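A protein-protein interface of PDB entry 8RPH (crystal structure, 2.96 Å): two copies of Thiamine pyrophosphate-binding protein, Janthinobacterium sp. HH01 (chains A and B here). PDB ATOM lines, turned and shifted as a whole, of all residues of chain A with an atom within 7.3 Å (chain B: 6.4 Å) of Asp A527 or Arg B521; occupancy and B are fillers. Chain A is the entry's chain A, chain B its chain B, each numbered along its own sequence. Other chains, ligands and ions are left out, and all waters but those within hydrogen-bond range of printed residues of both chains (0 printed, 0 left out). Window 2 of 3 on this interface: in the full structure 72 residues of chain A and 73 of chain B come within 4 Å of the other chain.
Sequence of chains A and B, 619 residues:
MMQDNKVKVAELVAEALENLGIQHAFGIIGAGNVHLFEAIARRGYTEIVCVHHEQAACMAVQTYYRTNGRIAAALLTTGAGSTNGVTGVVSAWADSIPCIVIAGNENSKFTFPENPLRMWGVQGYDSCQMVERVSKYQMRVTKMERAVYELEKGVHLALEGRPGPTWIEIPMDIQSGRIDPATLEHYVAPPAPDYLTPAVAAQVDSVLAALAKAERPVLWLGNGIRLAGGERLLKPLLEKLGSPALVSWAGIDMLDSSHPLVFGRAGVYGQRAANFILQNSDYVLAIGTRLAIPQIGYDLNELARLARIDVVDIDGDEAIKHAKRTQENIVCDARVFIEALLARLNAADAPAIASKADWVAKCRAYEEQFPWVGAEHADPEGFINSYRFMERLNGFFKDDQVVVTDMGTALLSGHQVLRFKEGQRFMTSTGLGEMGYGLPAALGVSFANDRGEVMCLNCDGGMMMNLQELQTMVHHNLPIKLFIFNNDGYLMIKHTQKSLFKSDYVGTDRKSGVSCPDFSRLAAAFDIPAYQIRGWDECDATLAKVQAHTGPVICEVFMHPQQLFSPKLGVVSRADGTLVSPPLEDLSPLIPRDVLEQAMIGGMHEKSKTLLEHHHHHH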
ATOM      1  N   VAL A 474      33.511  19.282  -1.874  1.00  0.00           N
ATOM      2  CA  VAL A 474      33.858  20.033  -0.674  1.00  0.00           C
ATOM      3  C   VAL A 474      35.364  20.238  -0.592  1.00  0.00           C
ATOM      4  O   VAL A 474      35.835  21.283  -0.128  1.00  0.00           O
ATOM      5  CB  VAL A 474      33.315  19.315   0.575  1.00  0.00           C
ATOM      6  CG1 VAL A 474      33.600  20.127   1.827  1.00  0.00           C
ATOM      7  CG2 VAL A 474      31.825  19.071   0.432  1.00  0.00           C
ATOM      8  N   ARG A 521      20.489  15.794   5.646  1.00  0.00           N
ATOM      9  CA  ARG A 521      21.342  15.271   6.707  1.00  0.00           C
ATOM     10  C   ARG A 521      22.694  14.845   6.152  1.00  0.00           C
ATOM     11  O   ARG A 521      23.744  15.159   6.724  1.00  0.00           O
ATOM     12  CB  ARG A 521      20.657  14.096   7.400  1.00  0.00           C
ATOM     13  CG  ARG A 521      19.310  14.437   7.997  1.00  0.00           C
ATOM     14  CD  ARG A 521      18.622  13.194   8.510  1.00  0.00           C
ATOM     15  NE  ARG A 521      19.449  12.474   9.471  1.00  0.00           N
ATOM     16  CZ  ARG A 521      19.160  11.274   9.954  1.00  0.00           C
ATOM     17  NH1 ARG A 521      18.078  10.616   9.570  1.00  0.00           N
ATOM     18  NH2 ARG A 521      19.980  10.718  10.841  1.00  0.00           N
ATOM     19  N   LEU A 522      22.685  14.126   5.028  1.00  0.00           N
ATOM     20  CA  LEU A 522      23.939  13.726   4.403  1.00  0.00           C
ATOM     21  C   LEU A 522      24.798  14.944   4.089  1.00  0.00           C
ATOM     22  O   LEU A 522      26.009  14.941   4.340  1.00  0.00           O
ATOM     23  CB  LEU A 522      23.651  12.919   3.135  1.00  0.00           C
ATOM     24  CG  LEU A 522      24.780  12.063   2.561  1.00  0.00           C
ATOM     25  CD1 LEU A 522      25.321  11.089   3.597  1.00  0.00           C
ATOM     26  CD2 LEU A 522      24.285  11.308   1.335  1.00  0.00           C
ATOM     27  N   ALA A 523      24.184  16.003   3.554  1.00  0.00           N
ATOM     28  CA  ALA A 523      24.927  17.227   3.275  1.00  0.00           C
ATOM     29  C   ALA A 523      25.601  17.760   4.532  1.00  0.00           C
ATOM     30  O   ALA A 523      26.772  18.155   4.498  1.00  0.00           O
ATOM     31  CB  ALA A 523      23.992  18.284   2.688  1.00  0.00           C
ATOM     32  N   ALA A 524      24.872  17.780   5.652  1.00  0.00           N
ATOM     33  CA  ALA A 524      25.448  18.255   6.906  1.00  0.00           C
ATOM     34  C   ALA A 524      26.696  17.467   7.269  1.00  0.00           C
ATOM     35  O   ALA A 524      27.655  18.026   7.814  1.00  0.00           O
ATOM     36  CB  ALA A 524      24.411  18.162   8.023  1.00  0.00           C
ATOM     37  N   ALA A 525      26.709  16.167   6.967  1.00  0.00           N
ATOM     38  CA  ALA A 525      27.888  15.357   7.249  1.00  0.00           C
ATOM     39  C   ALA A 525      29.078  15.811   6.411  1.00  0.00           C
ATOM     40  O   ALA A 525      30.212  15.847   6.902  1.00  0.00           O
ATOM     41  CB  ALA A 525      27.579  13.882   6.997  1.00  0.00           C
ATOM     42  N   PHE A 526      28.836  16.170   5.149  1.00  0.00           N
ATOM     43  CA  PHE A 526      29.873  16.668   4.254  1.00  0.00           C
ATOM     44  C   PHE A 526      30.158  18.160   4.431  1.00  0.00           C
ATOM     45  O   PHE A 526      30.889  18.733   3.616  1.00  0.00           O
ATOM     46  CB  PHE A 526      29.479  16.406   2.796  1.00  0.00           C
ATOM     47  CG  PHE A 526      29.666  14.978   2.353  1.00  0.00           C
ATOM     48  CD1 PHE A 526      30.925  14.490   2.049  1.00  0.00           C
ATOM     49  CD2 PHE A 526      28.579  14.133   2.219  1.00  0.00           C
ATOM     50  CE1 PHE A 526      31.100  13.183   1.635  1.00  0.00           C
ATOM     51  CE2 PHE A 526      28.746  12.827   1.800  1.00  0.00           C
ATOM     52  CZ  PHE A 526      30.008  12.352   1.511  1.00  0.00           C
ATOM     53  N   ASP A 527      29.605  18.806   5.460  1.00  0.00           N
ATOM     54  CA  ASP A 527      29.804  20.241   5.679  1.00  0.00           C
ATOM     55  C   ASP A 527      29.316  21.062   4.485  1.00  0.00           C
ATOM     56  O   ASP A 527      29.969  22.014   4.053  1.00  0.00           O
ATOM     57  CB  ASP A 527      31.274  20.552   5.980  1.00  0.00           C
ATOM     58  CG  ASP A 527      31.685  20.135   7.380  1.00  0.00           C
ATOM     59  OD1 ASP A 527      30.959  20.472   8.341  1.00  0.00           O
ATOM     60  OD2 ASP A 527      32.735  19.470   7.517  1.00  0.00           O
ATOM     61  N   ILE A 528      28.155  20.697   3.952  1.00  0.00           N
ATOM     62  CA  ILE A 528      27.550  21.371   2.809  1.00  0.00           C
ATOM     63  C   ILE A 528      26.232  21.984   3.269  1.00  0.00           C
ATOM     64  O   ILE A 528      25.360  21.264   3.765  1.00  0.00           O
ATOM     65  CB  ILE A 528      27.312  20.412   1.629  1.00  0.00           C
ATOM     66  CG1 ILE A 528      28.635  19.818   1.131  1.00  0.00           C
ATOM     67  CG2 ILE A 528      26.575  21.133   0.497  1.00  0.00           C
ATOM     68  CD1 ILE A 528      28.467  18.792   0.017  1.00  0.00           C
ATOM     69  N   PRO A 529      26.022  23.295   3.122  1.00  0.00           N
ATOM     70  CA  PRO A 529      24.719  23.863   3.489  1.00  0.00           C
ATOM     71  C   PRO A 529      23.605  23.245   2.658  1.00  0.00           C
ATOM     72  O   PRO A 529      23.768  22.987   1.463  1.00  0.00           O
ATOM     73  CB  PRO A 529      24.884  25.361   3.203  1.00  0.00           C
ATOM     74  CG  PRO A 529      26.028  25.458   2.257  1.00  0.00           C
ATOM     75  CD  PRO A 529      26.942  24.323   2.599  1.00  0.00           C
ATOM     76  N   ALA A 530      22.467  22.997   3.306  1.00  0.00           N
ATOM     77  CA  ALA A 530      21.356  22.292   2.683  1.00  0.00           C
ATOM     78  C   ALA A 530      20.054  23.048   2.902  1.00  0.00           C
ATOM     79  O   ALA A 530      19.839  23.650   3.958  1.00  0.00           O
ATOM     80  CB  ALA A 530      21.223  20.868   3.239  1.00  0.00           C
ATOM     81  N   PRO A 552      29.664  25.109  -2.290  1.00  0.00           N
ATOM     82  CA  PRO A 552      28.673  24.100  -2.674  1.00  0.00           C
ATOM     83  C   PRO A 552      27.416  24.203  -1.828  1.00  0.00           C
ATOM     84  O   PRO A 552      27.452  24.577  -0.654  1.00  0.00           O
ATOM     85  CB  PRO A 552      29.404  22.771  -2.438  1.00  0.00           C
ATOM     86  CG  PRO A 552      30.440  23.082  -1.421  1.00  0.00           C
ATOM     87  CD  PRO A 552      30.846  24.513  -1.640  1.00  0.00           C
ATOM     88  N   ASP B 518      34.210  12.619   7.350  1.00  0.00           N
ATOM     89  CA  ASP B 518      34.042  12.044   8.680  1.00  0.00           C
ATOM     90  C   ASP B 518      32.978  10.955   8.608  1.00  0.00           C
ATOM     91  O   ASP B 518      31.786  11.250   8.482  1.00  0.00           O
ATOM     92  CB  ASP B 518      33.655  13.139   9.671  1.00  0.00           C
ATOM     93  CG  ASP B 518      33.729  12.680  11.117  1.00  0.00           C
ATOM     94  OD1 ASP B 518      33.477  11.486  11.382  1.00  0.00           O
ATOM     95  OD2 ASP B 518      34.036  13.519  11.992  1.00  0.00           O
ATOM     96  N   PHE B 519      33.404   9.692   8.678  1.00  0.00           N
ATOM     97  CA  PHE B 519      32.464   8.589   8.511  1.00  0.00           C
ATOM     98  C   PHE B 519      31.537   8.422   9.708  1.00  0.00           C
ATOM     99  O   PHE B 519      30.455   7.842   9.561  1.00  0.00           O
ATOM    100  CB  PHE B 519      33.223   7.288   8.249  1.00  0.00           C
ATOM    101  CG  PHE B 519      33.965   7.277   6.945  1.00  0.00           C
ATOM    102  CD1 PHE B 519      33.288   7.094   5.750  1.00  0.00           C
ATOM    103  CD2 PHE B 519      35.336   7.451   6.913  1.00  0.00           C
ATOM    104  CE1 PHE B 519      33.967   7.084   4.547  1.00  0.00           C
ATOM    105  CE2 PHE B 519      36.020   7.443   5.713  1.00  0.00           C
ATOM    106  CZ  PHE B 519      35.335   7.261   4.529  1.00  0.00           C
ATOM    107  N   SER B 520      31.926   8.909  10.888  1.00  0.00           N
ATOM    108  CA  SER B 520      30.990   8.912  12.008  1.00  0.00           C
ATOM    109  C   SER B 520      29.827   9.858  11.738  1.00  0.00           C
ATOM    110  O   SER B 520      28.683   9.563  12.098  1.00  0.00           O
ATOM    111  CB  SER B 520      31.709   9.297  13.300  1.00  0.00           C
ATOM    112  OG  SER B 520      32.639   8.300  13.687  1.00  0.00           O
ATOM    113  N   ARG B 521      30.099  10.999  11.098  1.00  0.00           N
ATOM    114  CA  ARG B 521      29.034  11.942  10.773  1.00  0.00           C
ATOM    115  C   ARG B 521      28.209  11.478   9.581  1.00  0.00           C
ATOM    116  O   ARG B 521      27.025  11.820   9.484  1.00  0.00           O
ATOM    117  CB  ARG B 521      29.623  13.325  10.498  1.00  0.00           C
ATOM    118  CG  ARG B 521      30.284  13.963  11.709  1.00  0.00           C
ATOM    119  CD  ARG B 521      31.008  15.242  11.335  1.00  0.00           C
ATOM    120  NE  ARG B 521      30.113  16.238  10.758  1.00  0.00           N
ATOM    121  CZ  ARG B 521      30.513  17.396  10.250  1.00  0.00           C
ATOM    122  NH1 ARG B 521      31.792  17.736  10.227  1.00  0.00           N
ATOM    123  NH2 ARG B 521      29.608  18.234   9.753  1.00  0.00           N
ATOM    124  N   LEU B 522      28.811  10.717   8.663  1.00  0.00           N
ATOM    125  CA  LEU B 522      28.026  10.076   7.615  1.00  0.00           C
ATOM    126  C   LEU B 522      27.165   8.964   8.190  1.00  0.00           C
ATOM    127  O   LEU B 522      26.022   8.769   7.763  1.00  0.00           O
ATOM    128  CB  LEU B 522      28.941   9.515   6.528  1.00  0.00           C
ATOM    129  CG  LEU B 522      29.588  10.492   5.548  1.00  0.00           C
ATOM    130  CD1 LEU B 522      30.470   9.734   4.568  1.00  0.00           C
ATOM    131  CD2 LEU B 522      28.535  11.281   4.800  1.00  0.00           C
ATOM    132  N   ALA B 523      27.704   8.218   9.156  1.00  0.00           N
ATOM    133  CA  ALA B 523      26.925   7.165   9.793  1.00  0.00           C
ATOM    134  C   ALA B 523      25.653   7.729  10.408  1.00  0.00           C
ATOM    135  O   ALA B 523      24.570   7.150  10.263  1.00  0.00           O
ATOM    136  CB  ALA B 523      27.769   6.465  10.856  1.00  0.00           C
ATOM    137  N   ALA B 524      25.767   8.867  11.094  1.00  0.00           N
ATOM    138  CA  ALA B 524      24.587   9.507  11.663  1.00  0.00           C
ATOM    139  C   ALA B 524      23.578   9.854  10.576  1.00  0.00           C
ATOM    140  O   ALA B 524      22.366   9.703  10.771  1.00  0.00           O
ATOM    141  CB  ALA B 524      25.000  10.758  12.438  1.00  0.00           C
ATOM    142  N   ALA B 525      24.059  10.306   9.415  1.00  0.00           N
ATOM    143  CA  ALA B 525      23.149  10.693   8.343  1.00  0.00           C
ATOM    144  C   ALA B 525      22.387   9.489   7.804  1.00  0.00           C
ATOM    145  O   ALA B 525      21.210   9.605   7.435  1.00  0.00           O
ATOM    146  CB  ALA B 525      23.927  11.387   7.224  1.00  0.00           C
ATOM    147  N   PHE B 526      23.035   8.328   7.749  1.00  0.00           N
ATOM    148  CA  PHE B 526      22.406   7.089   7.316  1.00  0.00           C
ATOM    149  C   PHE B 526      21.689   6.361   8.447  1.00  0.00           C
ATOM    150  O   PHE B 526      21.260   5.219   8.254  1.00  0.00           O
ATOM    151  CB  PHE B 526      23.453   6.159   6.697  1.00  0.00           C
ATOM    152  CG  PHE B 526      23.890   6.568   5.322  1.00  0.00           C
ATOM    153  CD1 PHE B 526      23.099   6.287   4.220  1.00  0.00           C
ATOM    154  CD2 PHE B 526      25.092   7.226   5.128  1.00  0.00           C
ATOM    155  CE1 PHE B 526      23.496   6.660   2.952  1.00  0.00           C
ATOM    156  CE2 PHE B 526      25.495   7.600   3.860  1.00  0.00           C
ATOM    157  CZ  PHE B 526      24.695   7.316   2.772  1.00  0.00           C
ATOM    158  N   ALA B 530      27.592   4.777  15.289  1.00  0.00           N
ATOM    159  CA  ALA B 530      29.000   4.947  14.965  1.00  0.00           C
ATOM    160  C   ALA B 530      29.826   5.139  16.228  1.00  0.00           C
ATOM    161  O   ALA B 530      29.435   5.882  17.132  1.00  0.00           O
ATOM    162  CB  ALA B 530      29.214   6.144  14.037  1.00  0.00           C
ATOM    163  N   GLU B 556      35.165   3.879  13.385  1.00  0.00           N
ATOM    164  CA  GLU B 556      36.382   4.430  12.805  1.00  0.00           C
ATOM    165  C   GLU B 556      37.584   4.079  13.675  1.00  0.00           C
ATOM    166  O   GLU B 556      37.549   4.254  14.897  1.00  0.00           O
ATOM    167  CB  GLU B 556      36.272   5.948  12.664  1.00  0.00           C
ATOM    168  CG  GLU B 556      35.402   6.426  11.516  1.00  0.00           C
ATOM    169  CD  GLU B 556      35.297   7.941  11.470  1.00  0.00           C
ATOM    170  OE1 GLU B 556      34.885   8.540  12.487  1.00  0.00           O
ATOM    171  OE2 GLU B 556      35.641   8.534  10.426  1.00  0.00           O
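NH2 of Arg A521 sits at hydrogen-bond distance from O of Ala B524, at 2.6 Å.
O of Ala A524 lies within hydrogen-bond range of NH2 of Arg B521, 2.8 Å away.
The guanidinium group (NH2) of Arg B521 is in salt-bridge range of the side-chain carboxylate (OD1) of Asp A527 (3.0 Å).
N of Arg B521 lies within hydrogen-bond range of OD1 of Asp B518, 3.4 Å away.
O of Ala B525 touches CZ of Arg A521, at 3.7 Å.
Leu B522 touches Leu A522.
Ala B525 touches Leu A522 (CB to CA, 3.7 Å).
Leu A522 touches Phe B526.
O of Arg B521 touches CB of Ala A525 (3.3 Å).
Leu B522 touches Ala A525 (CD2 to CB, 3.5 Å).
Phe A526 touches Leu B522.
Of chain B, only Arg B521 comes within 4 Å of Asp A527.
Of chain A, only Ala A524 (2.8 Å), Ala A525 (3.3 Å) and Asp A527 (3.0 Å) come within 4 Å of Arg B521.
Of the printed residues of chain B, Phe A526 touches Leu B522 (3.4 Å).
Printed residues of chain A within 4 Å of Leu B522: Leu A522 (3.4 Å), Ala A525 (3.5 Å) and Phe A526 (3.4 Å).
Printed residues of chain B within 4 Å of Ala A524: Arg B521 (2.8 Å).
Ala A523 touches none of the printed residues of chain B.
The nearest printed residue of chain A that does not touch Phe B526 is Arg A521 (5.0 Å).
Printed residues of chain B that touch a printed residue of chain A: Arg B521, Leu B522, Ala B524, Ala B525 and Phe B526.
Hydrophobic or aromatic side chains of chain B within 4 Å of the printed part of chain A: Leu B522, Ala B525 and Phe B526.
Of the 12 printed residues of chain A, 6 touch a printed residue of chain B.
Among the printed residues, 10 pairs touch across the chains.
Among the printed residues, Asp or Glu carboxylates within 4 Å of a Lys or Arg side-chain nitrogen of the other chain: Asp A527 with Arg B521 (3.0 Å).
Arg A521 touches Ala B524, and with the chains exchanged Ala A524 touches Arg B521.
Leu B522 touches its own counterpart, Leu A522.
Leu A522 touches Ala B525, and with the chains exchanged Ala A525 touches Leu B522.
Leu A522 touches Phe B526, and with the chains exchanged Phe A526 touches Leu B522.
7 positions are printed for both chains.
Of the 10 pairs that touch across the chains among the printed residues, 9 have their exchanged pair printed and touching as well.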
